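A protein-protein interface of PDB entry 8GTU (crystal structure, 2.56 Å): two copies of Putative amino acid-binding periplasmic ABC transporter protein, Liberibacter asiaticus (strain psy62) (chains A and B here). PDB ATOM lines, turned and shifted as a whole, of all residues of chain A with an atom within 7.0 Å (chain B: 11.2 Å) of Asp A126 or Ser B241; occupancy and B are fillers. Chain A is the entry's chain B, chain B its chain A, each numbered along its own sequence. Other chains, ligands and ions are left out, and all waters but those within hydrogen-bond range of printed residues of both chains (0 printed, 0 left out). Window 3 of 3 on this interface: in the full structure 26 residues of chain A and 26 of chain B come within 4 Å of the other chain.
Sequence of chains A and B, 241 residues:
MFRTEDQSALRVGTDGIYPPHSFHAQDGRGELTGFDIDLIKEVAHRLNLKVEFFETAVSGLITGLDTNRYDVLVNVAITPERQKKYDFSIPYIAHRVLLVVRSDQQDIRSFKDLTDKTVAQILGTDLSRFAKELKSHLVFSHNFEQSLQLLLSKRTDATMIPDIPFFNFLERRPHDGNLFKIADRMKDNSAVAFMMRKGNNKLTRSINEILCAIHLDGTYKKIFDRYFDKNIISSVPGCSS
The backbone NH (N) of Ser B240 is in hydrogen-bond range of the backbone carbonyl oxygen (O) of Ile A78, 3.2 Å away.
The side-chain carboxylate (OD2) of Asp A126 sits close to the backbone carbonyl oxygen (O) of Ser B241 (2.8 Å).
The side-chain hydroxyl (OG1) of Thr A79 lies within hydrogen-bond range of the backbone NH (N) of Arg A82, 3.2 Å away.
The side-chain sulfur (SG) of Cys B212 forms a disulfide with the side-chain sulfur (SG) of Cys B239 (2.1 Å).
The side-chain carboxylate (OD1) of Asp A126 is in salt-bridge range of the guanidinium group (NH2) of Arg A82, at 2.9 Å.
The backbone carbonyl oxygen (O) of Ala A77 lies within hydrogen-bond range of the guanidinium group (NH1) of Arg A82, at 2.8 Å.
Among the printed residues, merely in contact across the chains: Thr A79 with Ser B240 (3.2 Å), Pro A80 with Ser B240 (3.4 Å), Ala A77 with Ser B240 (3.6 Å), Ser A190 with Ser B240 (3.6 Å), Pro A80 with Leu B216 (3.7 Å), Pro A80 with Glu B209 (3.8 Å), Ile A78 with Cys B239 (3.8 Å), Ile A78 with Cys B212 (3.8 Å), Thr A79 with Ser B241 (3.9 Å) and Ser A190 with Gly B238 (3.95 Å).
No position is printed for both chains.
Of the 12 pairs that touch across the chains among the printed residues, none has its exchanged pair printed and touching as well.
Printed residues of chain A that touch a printed residue of chain B: Ala A77, Ile A78, Thr A79, Pro A80, Asp A126 and Ser A190.
Hydrophobic or aromatic side chains of chain A within 4 Å of the printed part of chain B: Ala A77, Ile A78 and Pro A80.
Hydrophobic or aromatic side chains of chain B that line the printed part of chain A: Leu B216.
Among the printed residues, 12 pairs touch across the chains.
Among the printed residues, no Asp or Glu carboxylate lies within 4 Å of a Lys or Arg side-chain nitrogen of the other chain.
Asp A126 touches one residue of chain B.
No residue of chain B comes within 4 Å of Gly A124.
No residue of chain B comes within 4 Å of Leu A127.
Of the printed residues of chain B, Pro A80 touches Glu B209, Leu B216 and Ser B240.
Of the printed residues of chain A, Gly B238 touches Ser A190 (3.95 Å).
Arg A82 touches none of the printed residues of chain B.
Ala B213 touches none of the printed residues of chain A.
The nearest residue of chain B that does not touch Asp A126 is Ser B240 (5.5 Å).
The nearest printed residue of chain A that does not touch Ser B241 is Pro A80 (4.2 Å).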
ATOM      1  N   ILE A  62      18.320  -8.864  -8.856  1.00  0.00           N
ATOM      2  CA  ILE A  62      18.398  -7.811  -7.848  1.00  0.00           C
ATOM      3  C   ILE A  62      18.086  -6.465  -8.516  1.00  0.00           C
ATOM      4  O   ILE A  62      17.428  -5.615  -7.921  1.00  0.00           O
ATOM      5  CB  ILE A  62      19.751  -7.884  -7.094  1.00  0.00           C
ATOM      6  CG1 ILE A  62      19.818  -9.168  -6.246  1.00  0.00           C
ATOM      7  CG2 ILE A  62      20.047  -6.638  -6.266  1.00  0.00           C
ATOM      8  CD1 ILE A  62      21.051  -9.347  -5.351  1.00  0.00           C
ATOM      9  N   ALA A  77      20.695 -15.864  -0.582  1.00  0.00           N
ATOM     10  CA  ALA A  77      21.589 -15.961   0.569  1.00  0.00           C
ATOM     11  C   ALA A  77      21.668 -14.621   1.301  1.00  0.00           C
ATOM     12  O   ALA A  77      21.875 -13.580   0.679  1.00  0.00           O
ATOM     13  CB  ALA A  77      22.946 -16.456   0.168  1.00  0.00           C
ATOM     14  N   ILE A  78      21.438 -14.676   2.618  1.00  0.00           N
ATOM     15  CA  ILE A  78      21.604 -13.552   3.523  1.00  0.00           C
ATOM     16  C   ILE A  78      23.101 -13.241   3.678  1.00  0.00           C
ATOM     17  O   ILE A  78      23.906 -14.092   4.038  1.00  0.00           O
ATOM     18  CB  ILE A  78      20.907 -13.847   4.874  1.00  0.00           C
ATOM     19  CG1 ILE A  78      19.394 -14.071   4.741  1.00  0.00           C
ATOM     20  CG2 ILE A  78      21.233 -12.783   5.899  1.00  0.00           C
ATOM     21  CD1 ILE A  78      18.678 -14.454   6.021  1.00  0.00           C
ATOM     22  N   THR A  79      23.477 -12.003   3.372  1.00  0.00           N
ATOM     23  CA  THR A  79      24.840 -11.517   3.536  1.00  0.00           C
ATOM     24  C   THR A  79      24.713 -10.184   4.263  1.00  0.00           C
ATOM     25  O   THR A  79      23.661  -9.567   4.167  1.00  0.00           O
ATOM     26  CB  THR A  79      25.551 -11.389   2.178  1.00  0.00           C
ATOM     27  OG1 THR A  79      25.053 -10.215   1.536  1.00  0.00           O
ATOM     28  CG2 THR A  79      25.329 -12.569   1.249  1.00  0.00           C
ATOM     29  N   PRO A  80      25.726  -9.692   5.013  1.00  0.00           N
ATOM     30  CA  PRO A  80      25.579  -8.439   5.749  1.00  0.00           C
ATOM     31  C   PRO A  80      25.384  -7.232   4.828  1.00  0.00           C
ATOM     32  O   PRO A  80      24.716  -6.280   5.214  1.00  0.00           O
ATOM     33  CB  PRO A  80      26.897  -8.290   6.535  1.00  0.00           C
ATOM     34  CG  PRO A  80      27.572  -9.640   6.444  1.00  0.00           C
ATOM     35  CD  PRO A  80      27.080 -10.257   5.151  1.00  0.00           C
ATOM     36  N   GLU A  81      25.991  -7.281   3.628  1.00  0.00           N
ATOM     37  CA  GLU A  81      25.884  -6.264   2.586  1.00  0.00           C
ATOM     38  C   GLU A  81      24.431  -6.134   2.136  1.00  0.00           C
ATOM     39  O   GLU A  81      23.900  -5.025   2.061  1.00  0.00           O
ATOM     40  CB  GLU A  81      26.862  -6.614   1.454  1.00  0.00           C
ATOM     41  CG  GLU A  81      26.618  -5.991   0.084  1.00  0.00           C
ATOM     42  CD  GLU A  81      27.776  -6.254  -0.875  1.00  0.00           C
ATOM     43  OE1 GLU A  81      28.912  -5.827  -0.561  1.00  0.00           O
ATOM     44  OE2 GLU A  81      27.558  -6.901  -1.925  1.00  0.00           O
ATOM     45  N   ARG A  82      23.800  -7.283   1.850  1.00  0.00           N
ATOM     46  CA  ARG A  82      22.395  -7.360   1.474  1.00  0.00           C
ATOM     47  C   ARG A  82      21.486  -7.010   2.661  1.00  0.00           C
ATOM     48  O   ARG A  82      20.405  -6.440   2.469  1.00  0.00           O
ATOM     49  CB  ARG A  82      22.042  -8.747   0.929  1.00  0.00           C
ATOM     50  CG  ARG A  82      22.549  -9.042  -0.472  1.00  0.00           C
ATOM     51  CD  ARG A  82      22.320 -10.494  -0.857  1.00  0.00           C
ATOM     52  NE  ARG A  82      22.908 -10.826  -2.150  1.00  0.00           N
ATOM     53  CZ  ARG A  82      23.358 -12.034  -2.524  1.00  0.00           C
ATOM     54  NH1 ARG A  82      23.112 -13.107  -1.780  1.00  0.00           N
ATOM     55  NH2 ARG A  82      24.027 -12.163  -3.667  1.00  0.00           N
ATOM     56  N   GLN A 121      31.019 -20.014 -13.416  1.00  0.00           N
ATOM     57  CA  GLN A 121      30.158 -19.386 -12.427  1.00  0.00           C
ATOM     58  C   GLN A 121      29.102 -18.559 -13.143  1.00  0.00           C
ATOM     59  O   GLN A 121      29.258 -18.229 -14.316  1.00  0.00           O
ATOM     60  CB  GLN A 121      30.936 -18.479 -11.463  1.00  0.00           C
ATOM     61  CG  GLN A 121      32.105 -19.131 -10.715  1.00  0.00           C
ATOM     62  CD  GLN A 121      31.719 -20.206  -9.725  1.00  0.00           C
ATOM     63  OE1 GLN A 121      32.434 -21.182  -9.507  1.00  0.00           O
ATOM     64  NE2 GLN A 121      30.578 -20.032  -9.087  1.00  0.00           N
ATOM     65  N   ILE A 122      28.048 -18.193 -12.408  1.00  0.00           N
ATOM     66  CA  ILE A 122      26.962 -17.408 -12.961  1.00  0.00           C
ATOM     67  C   ILE A 122      27.240 -15.925 -12.747  1.00  0.00           C
ATOM     68  O   ILE A 122      27.600 -15.508 -11.648  1.00  0.00           O
ATOM     69  CB  ILE A 122      25.595 -17.899 -12.437  1.00  0.00           C
ATOM     70  CG1 ILE A 122      25.433 -19.383 -12.793  1.00  0.00           C
ATOM     71  CG2 ILE A 122      24.419 -17.077 -12.993  1.00  0.00           C
ATOM     72  CD1 ILE A 122      24.996 -20.209 -11.636  1.00  0.00           C
ATOM     73  N   GLY A 124      27.051 -12.120 -12.072  1.00  0.00           N
ATOM     74  CA  GLY A 124      26.388 -11.319 -11.055  1.00  0.00           C
ATOM     75  C   GLY A 124      26.014 -12.101  -9.796  1.00  0.00           C
ATOM     76  O   GLY A 124      24.969 -11.838  -9.203  1.00  0.00           O
ATOM     77  N   THR A 125      26.837 -13.077  -9.399  1.00  0.00           N
ATOM     78  CA  THR A 125      26.596 -13.749  -8.136  1.00  0.00           C
ATOM     79  C   THR A 125      27.805 -13.541  -7.230  1.00  0.00           C
ATOM     80  O   THR A 125      28.882 -13.221  -7.710  1.00  0.00           O
ATOM     81  CB  THR A 125      26.241 -15.228  -8.330  1.00  0.00           C
ATOM     82  OG1 THR A 125      27.365 -15.869  -8.928  1.00  0.00           O
ATOM     83  CG2 THR A 125      24.999 -15.463  -9.161  1.00  0.00           C
ATOM     84  N   ASP A 126      27.601 -13.715  -5.920  1.00  0.00           N
ATOM     85  CA  ASP A 126      28.637 -13.635  -4.902  1.00  0.00           C
ATOM     86  C   ASP A 126      29.760 -14.655  -5.169  1.00  0.00           C
ATOM     87  O   ASP A 126      30.943 -14.358  -5.001  1.00  0.00           O
ATOM     88  CB  ASP A 126      28.001 -13.645  -3.501  1.00  0.00           C
ATOM     89  CG  ASP A 126      27.425 -12.308  -3.019  1.00  0.00           C
ATOM     90  OD1 ASP A 126      26.869 -11.539  -3.841  1.00  0.00           O
ATOM     91  OD2 ASP A 126      27.550 -12.022  -1.808  1.00  0.00           O
ATOM     92  N   LEU A 127      29.393 -15.849  -5.622  1.00  0.00           N
ATOM     93  CA  LEU A 127      30.357 -16.894  -5.929  1.00  0.00           C
ATOM     94  C   LEU A 127      31.199 -16.504  -7.140  1.00  0.00           C
ATOM     95  O   LEU A 127      32.365 -16.889  -7.248  1.00  0.00           O
ATOM     96  CB  LEU A 127      29.617 -18.210  -6.192  1.00  0.00           C
ATOM     97  CG  LEU A 127      29.095 -18.931  -4.952  1.00  0.00           C
ATOM     98  CD1 LEU A 127      28.476 -20.256  -5.343  1.00  0.00           C
ATOM     99  CD2 LEU A 127      30.222 -19.146  -3.945  1.00  0.00           C
ATOM    100  N   SER A 128      30.579 -15.746  -8.050  1.00  0.00           N
ATOM    101  CA  SER A 128      31.257 -15.227  -9.223  1.00  0.00           C
ATOM    102  C   SER A 128      32.273 -14.166  -8.787  1.00  0.00           C
ATOM    103  O   SER A 128      33.349 -14.046  -9.370  1.00  0.00           O
ATOM    104  CB  SER A 128      30.248 -14.678 -10.188  1.00  0.00           C
ATOM    105  OG  SER A 128      30.794 -14.589 -11.488  1.00  0.00           O
ATOM    106  N   ARG A 129      31.915 -13.407  -7.749  1.00  0.00           N
ATOM    107  CA  ARG A 129      32.767 -12.346  -7.252  1.00  0.00           C
ATOM    108  C   ARG A 129      33.907 -12.915  -6.429  1.00  0.00           C
ATOM    109  O   ARG A 129      35.024 -12.397  -6.491  1.00  0.00           O
ATOM    110  CB  ARG A 129      32.033 -11.144  -6.663  1.00  0.00           C
ATOM    111  CG  ARG A 129      32.408  -9.946  -7.529  1.00  0.00           C
ATOM    112  CD  ARG A 129      32.798  -8.533  -7.121  1.00  0.00           C
ATOM    113  NE  ARG A 129      34.176  -8.204  -6.725  1.00  0.00           N
ATOM    114  CZ  ARG A 129      34.501  -7.865  -5.482  1.00  0.00           C
ATOM    115  NH1 ARG A 129      33.574  -7.935  -4.542  1.00  0.00           N
ATOM    116  NH2 ARG A 129      35.738  -7.508  -5.183  1.00  0.00           N
ATOM    117  N   PHE A 130      33.610 -14.020  -5.734  1.00  0.00           N
ATOM    118  CA  PHE A 130      34.611 -14.731  -4.965  1.00  0.00           C
ATOM    119  C   PHE A 130      35.660 -15.324  -5.905  1.00  0.00           C
ATOM    120  O   PHE A 130      36.865 -15.275  -5.617  1.00  0.00           O
ATOM    121  CB  PHE A 130      33.962 -15.784  -4.065  1.00  0.00           C
ATOM    122  CG  PHE A 130      34.954 -16.517  -3.203  1.00  0.00           C
ATOM    123  CD1 PHE A 130      35.975 -15.834  -2.554  1.00  0.00           C
ATOM    124  CD2 PHE A 130      34.884 -17.894  -3.054  1.00  0.00           C
ATOM    125  CE1 PHE A 130      36.911 -16.504  -1.781  1.00  0.00           C
ATOM    126  CE2 PHE A 130      35.826 -18.565  -2.279  1.00  0.00           C
ATOM    127  CZ  PHE A 130      36.831 -17.869  -1.645  1.00  0.00           C
ATOM    128  N   ALA A 131      35.173 -15.871  -7.030  1.00  0.00           N
ATOM    129  CA  ALA A 131      36.031 -16.395  -8.082  1.00  0.00           C
ATOM    130  C   ALA A 131      36.951 -15.292  -8.633  1.00  0.00           C
ATOM    131  O   ALA A 131      38.135 -15.525  -8.837  1.00  0.00           O
ATOM    132  CB  ALA A 131      35.169 -17.054  -9.132  1.00  0.00           C
ATOM    133  N   LYS A 132      36.402 -14.088  -8.850  1.00  0.00           N
ATOM    134  CA  LYS A 132      37.136 -12.903  -9.286  1.00  0.00           C
ATOM    135  C   LYS A 132      38.268 -12.550  -8.317  1.00  0.00           C
ATOM    136  O   LYS A 132      39.392 -12.351  -8.765  1.00  0.00           O
ATOM    137  CB  LYS A 132      36.187 -11.726  -9.524  1.00  0.00           C
ATOM    138  CG  LYS A 132      35.748 -11.475 -10.965  1.00  0.00           C
ATOM    139  CD  LYS A 132      34.273 -11.071 -11.023  1.00  0.00           C
ATOM    140  CE  LYS A 132      33.779 -10.592 -12.372  1.00  0.00           C
ATOM    141  NZ  LYS A 132      34.716  -9.644 -13.023  1.00  0.00           N
ATOM    142  N   GLU A 133      37.982 -12.493  -7.003  1.00  0.00           N
ATOM    143  CA  GLU A 133      38.971 -12.202  -5.967  1.00  0.00           C
ATOM    144  C   GLU A 133      40.056 -13.272  -5.905  1.00  0.00           C
ATOM    145  O   GLU A 133      41.196 -12.976  -5.548  1.00  0.00           O
ATOM    146  CB  GLU A 133      38.329 -12.205  -4.578  1.00  0.00           C
ATOM    147  CG  GLU A 133      37.720 -10.874  -4.177  1.00  0.00           C
ATOM    148  CD  GLU A 133      36.358 -10.943  -3.483  1.00  0.00           C
ATOM    149  OE1 GLU A 133      36.184 -11.834  -2.634  1.00  0.00           O
ATOM    150  OE2 GLU A 133      35.461 -10.099  -3.795  1.00  0.00           O
ATOM    151  N   MET A 160      32.073 -23.710  -8.174  1.00  0.00           N
ATOM    152  CA  MET A 160      31.574 -23.567  -6.812  1.00  0.00           C
ATOM    153  C   MET A 160      30.056 -23.526  -6.923  1.00  0.00           C
ATOM    154  O   MET A 160      29.509 -22.693  -7.640  1.00  0.00           O
ATOM    155  CB  MET A 160      32.080 -22.261  -6.185  1.00  0.00           C
ATOM    156  CG  MET A 160      33.596 -22.238  -6.072  1.00  0.00           C
ATOM    157  SD  MET A 160      34.340 -20.797  -5.258  1.00  0.00           S
ATOM    158  CE  MET A 160      34.479 -19.670  -6.643  1.00  0.00           C
ATOM    159  N   SER A 190      24.706 -21.782   4.966  1.00  0.00           N
ATOM    160  CA  SER A 190      24.245 -20.429   4.718  1.00  0.00           C
ATOM    161  C   SER A 190      22.725 -20.362   4.779  1.00  0.00           C
ATOM    162  O   SER A 190      22.068 -21.067   4.037  1.00  0.00           O
ATOM    163  CB  SER A 190      24.686 -19.986   3.351  1.00  0.00           C
ATOM    164  OG  SER A 190      26.095 -19.904   3.277  1.00  0.00           O
ATOM    165  N   GLU B 209      22.412  -7.264  10.785  1.00  0.00           N
ATOM    166  CA  GLU B 209      23.653  -6.958  10.110  1.00  0.00           C
ATOM    167  C   GLU B 209      24.802  -7.446  10.983  1.00  0.00           C
ATOM    168  O   GLU B 209      25.674  -8.159  10.501  1.00  0.00           O
ATOM    169  CB  GLU B 209      23.728  -5.441  10.009  1.00  0.00           C
ATOM    170  CG  GLU B 209      24.051  -4.908   8.655  1.00  0.00           C
ATOM    171  CD  GLU B 209      23.928  -3.392   8.707  1.00  0.00           C
ATOM    172  OE1 GLU B 209      22.758  -2.872   8.728  1.00  0.00           O
ATOM    173  OE2 GLU B 209      24.997  -2.730   8.783  1.00  0.00           O
ATOM    174  N   LEU B 211      24.741  -9.466  13.691  1.00  0.00           N
ATOM    175  CA  LEU B 211      24.721 -10.896  13.952  1.00  0.00           C
ATOM    176  C   LEU B 211      25.370 -11.666  12.806  1.00  0.00           C
ATOM    177  O   LEU B 211      26.032 -12.677  13.029  1.00  0.00           O
ATOM    178  CB  LEU B 211      23.286 -11.372  14.195  1.00  0.00           C
ATOM    179  CG  LEU B 211      22.785 -11.147  15.620  1.00  0.00           C
ATOM    180  CD1 LEU B 211      21.300 -11.444  15.716  1.00  0.00           C
ATOM    181  CD2 LEU B 211      23.570 -12.030  16.573  1.00  0.00           C
ATOM    182  N   CYS B 212      25.167 -11.199  11.573  1.00  0.00           N
ATOM    183  CA  CYS B 212      25.707 -11.938  10.449  1.00  0.00           C
ATOM    184  C   CYS B 212      27.220 -11.764  10.388  1.00  0.00           C
ATOM    185  O   CYS B 212      27.937 -12.707  10.066  1.00  0.00           O
ATOM    186  CB  CYS B 212      24.979 -11.627   9.152  1.00  0.00           C
ATOM    187  SG  CYS B 212      23.533 -12.697   8.933  1.00  0.00           S
ATOM    188  N   ALA B 213      27.693 -10.571  10.772  1.00  0.00           N
ATOM    189  CA  ALA B 213      29.121 -10.295  10.896  1.00  0.00           C
ATOM    190  C   ALA B 213      29.764 -11.178  11.968  1.00  0.00           C
ATOM    191  O   ALA B 213      30.916 -11.588  11.836  1.00  0.00           O
ATOM    192  CB  ALA B 213      29.341  -8.835  11.201  1.00  0.00           C
ATOM    193  N   ILE B 214      29.016 -11.442  13.041  1.00  0.00           N
ATOM    194  CA  ILE B 214      29.492 -12.205  14.178  1.00  0.00           C
ATOM    195  C   ILE B 214      29.521 -13.678  13.787  1.00  0.00           C
ATOM    196  O   ILE B 214      30.424 -14.395  14.216  1.00  0.00           O
ATOM    197  CB  ILE B 214      28.639 -11.911  15.432  1.00  0.00           C
ATOM    198  CG1 ILE B 214      28.989 -10.545  16.026  1.00  0.00           C
ATOM    199  CG2 ILE B 214      28.769 -13.022  16.463  1.00  0.00           C
ATOM    200  CD1 ILE B 214      28.060 -10.054  17.114  1.00  0.00           C
ATOM    201  N   HIS B 215      28.557 -14.119  12.959  1.00  0.00           N
ATOM    202  CA  HIS B 215      28.657 -15.443  12.360  1.00  0.00           C
ATOM    203  C   HIS B 215      29.973 -15.534  11.594  1.00  0.00           C
ATOM    204  O   HIS B 215      30.744 -16.459  11.824  1.00  0.00           O
ATOM    205  CB  HIS B 215      27.437 -15.868  11.526  1.00  0.00           C
ATOM    206  CG  HIS B 215      26.270 -16.378  12.309  1.00  0.00           C
ATOM    207  ND1 HIS B 215      26.148 -17.689  12.724  1.00  0.00           N
ATOM    208  CD2 HIS B 215      25.142 -15.756  12.712  1.00  0.00           C
ATOM    209  CE1 HIS B 215      25.001 -17.836  13.393  1.00  0.00           C
ATOM    210  NE2 HIS B 215      24.372 -16.668  13.404  1.00  0.00           N
ATOM    211  N   LEU B 216      30.253 -14.541  10.746  1.00  0.00           N
ATOM    212  CA  LEU B 216      31.264 -14.661   9.711  1.00  0.00           C
ATOM    213  C   LEU B 216      32.692 -14.623  10.252  1.00  0.00           C
ATOM    214  O   LEU B 216      33.574 -15.168   9.600  1.00  0.00           O
ATOM    215  CB  LEU B 216      31.043 -13.560   8.678  1.00  0.00           C
ATOM    216  CG  LEU B 216      29.928 -13.835   7.675  1.00  0.00           C
ATOM    217  CD1 LEU B 216      29.778 -12.636   6.757  1.00  0.00           C
ATOM    218  CD2 LEU B 216      30.262 -15.078   6.866  1.00  0.00           C
ATOM    219  N   ASP B 217      32.932 -13.996  11.416  1.00  0.00           N
ATOM    220  CA  ASP B 217      34.300 -13.797  11.895  1.00  0.00           C
ATOM    221  C   ASP B 217      34.657 -14.774  13.022  1.00  0.00           C
ATOM    222  O   ASP B 217      35.687 -14.618  13.669  1.00  0.00           O
ATOM    223  CB  ASP B 217      34.607 -12.336  12.259  1.00  0.00           C
ATOM    224  CG  ASP B 217      34.043 -11.861  13.592  1.00  0.00           C
ATOM    225  OD1 ASP B 217      33.593 -12.705  14.401  1.00  0.00           O
ATOM    226  OD2 ASP B 217      34.034 -10.637  13.825  1.00  0.00           O
ATOM    227  N   GLY B 218      33.803 -15.768  13.267  1.00  0.00           N
ATOM    228  CA  GLY B 218      34.096 -16.804  14.240  1.00  0.00           C
ATOM    229  C   GLY B 218      33.657 -16.456  15.658  1.00  0.00           C
ATOM    230  O   GLY B 218      33.740 -17.320  16.525  1.00  0.00           O
ATOM    231  N   GLY B 238      24.637 -20.305   9.258  1.00  0.00           N
ATOM    232  CA  GLY B 238      25.494 -19.127   9.240  1.00  0.00           C
ATOM    233  C   GLY B 238      25.014 -18.067   8.247  1.00  0.00           C
ATOM    234  O   GLY B 238      23.846 -18.058   7.855  1.00  0.00           O
ATOM    235  N   CYS B 239      25.899 -17.128   7.887  1.00  0.00           N
ATOM    236  CA  CYS B 239      25.627 -16.150   6.841  1.00  0.00           C
ATOM    237  C   CYS B 239      26.714 -16.324   5.779  1.00  0.00           C
ATOM    238  O   CYS B 239      27.664 -17.059   6.013  1.00  0.00           O
ATOM    239  CB  CYS B 239      25.491 -14.736   7.413  1.00  0.00           C
ATOM    240  SG  CYS B 239      24.293 -14.617   8.784  1.00  0.00           S
ATOM    241  N   SER B 240      26.554 -15.724   4.598  1.00  0.00           N
ATOM    242  CA  SER B 240      27.616 -15.719   3.602  1.00  0.00           C
ATOM    243  C   SER B 240      27.947 -14.277   3.204  1.00  0.00           C
ATOM    244  O   SER B 240      27.463 -13.361   3.830  1.00  0.00           O
ATOM    245  CB  SER B 240      27.335 -16.649   2.440  1.00  0.00           C
ATOM    246  OG  SER B 240      26.105 -16.343   1.812  1.00  0.00           O
ATOM    247  N   SER B 241      28.789 -14.037   2.193  1.00  0.00           N
ATOM    248  CA  SER B 241      29.197 -12.659   1.931  1.00  0.00           C
ATOM    249  C   SER B 241      29.748 -12.442   0.510  1.00  0.00           C
ATOM    250  O   SER B 241      29.569 -13.339  -0.347  1.00  0.00           O
ATOM    251  CB  SER B 241      30.165 -12.170   2.992  1.00  0.00           C
ATOM    252  OG  SER B 241      31.158 -13.153   3.255  1.00  0.00           O
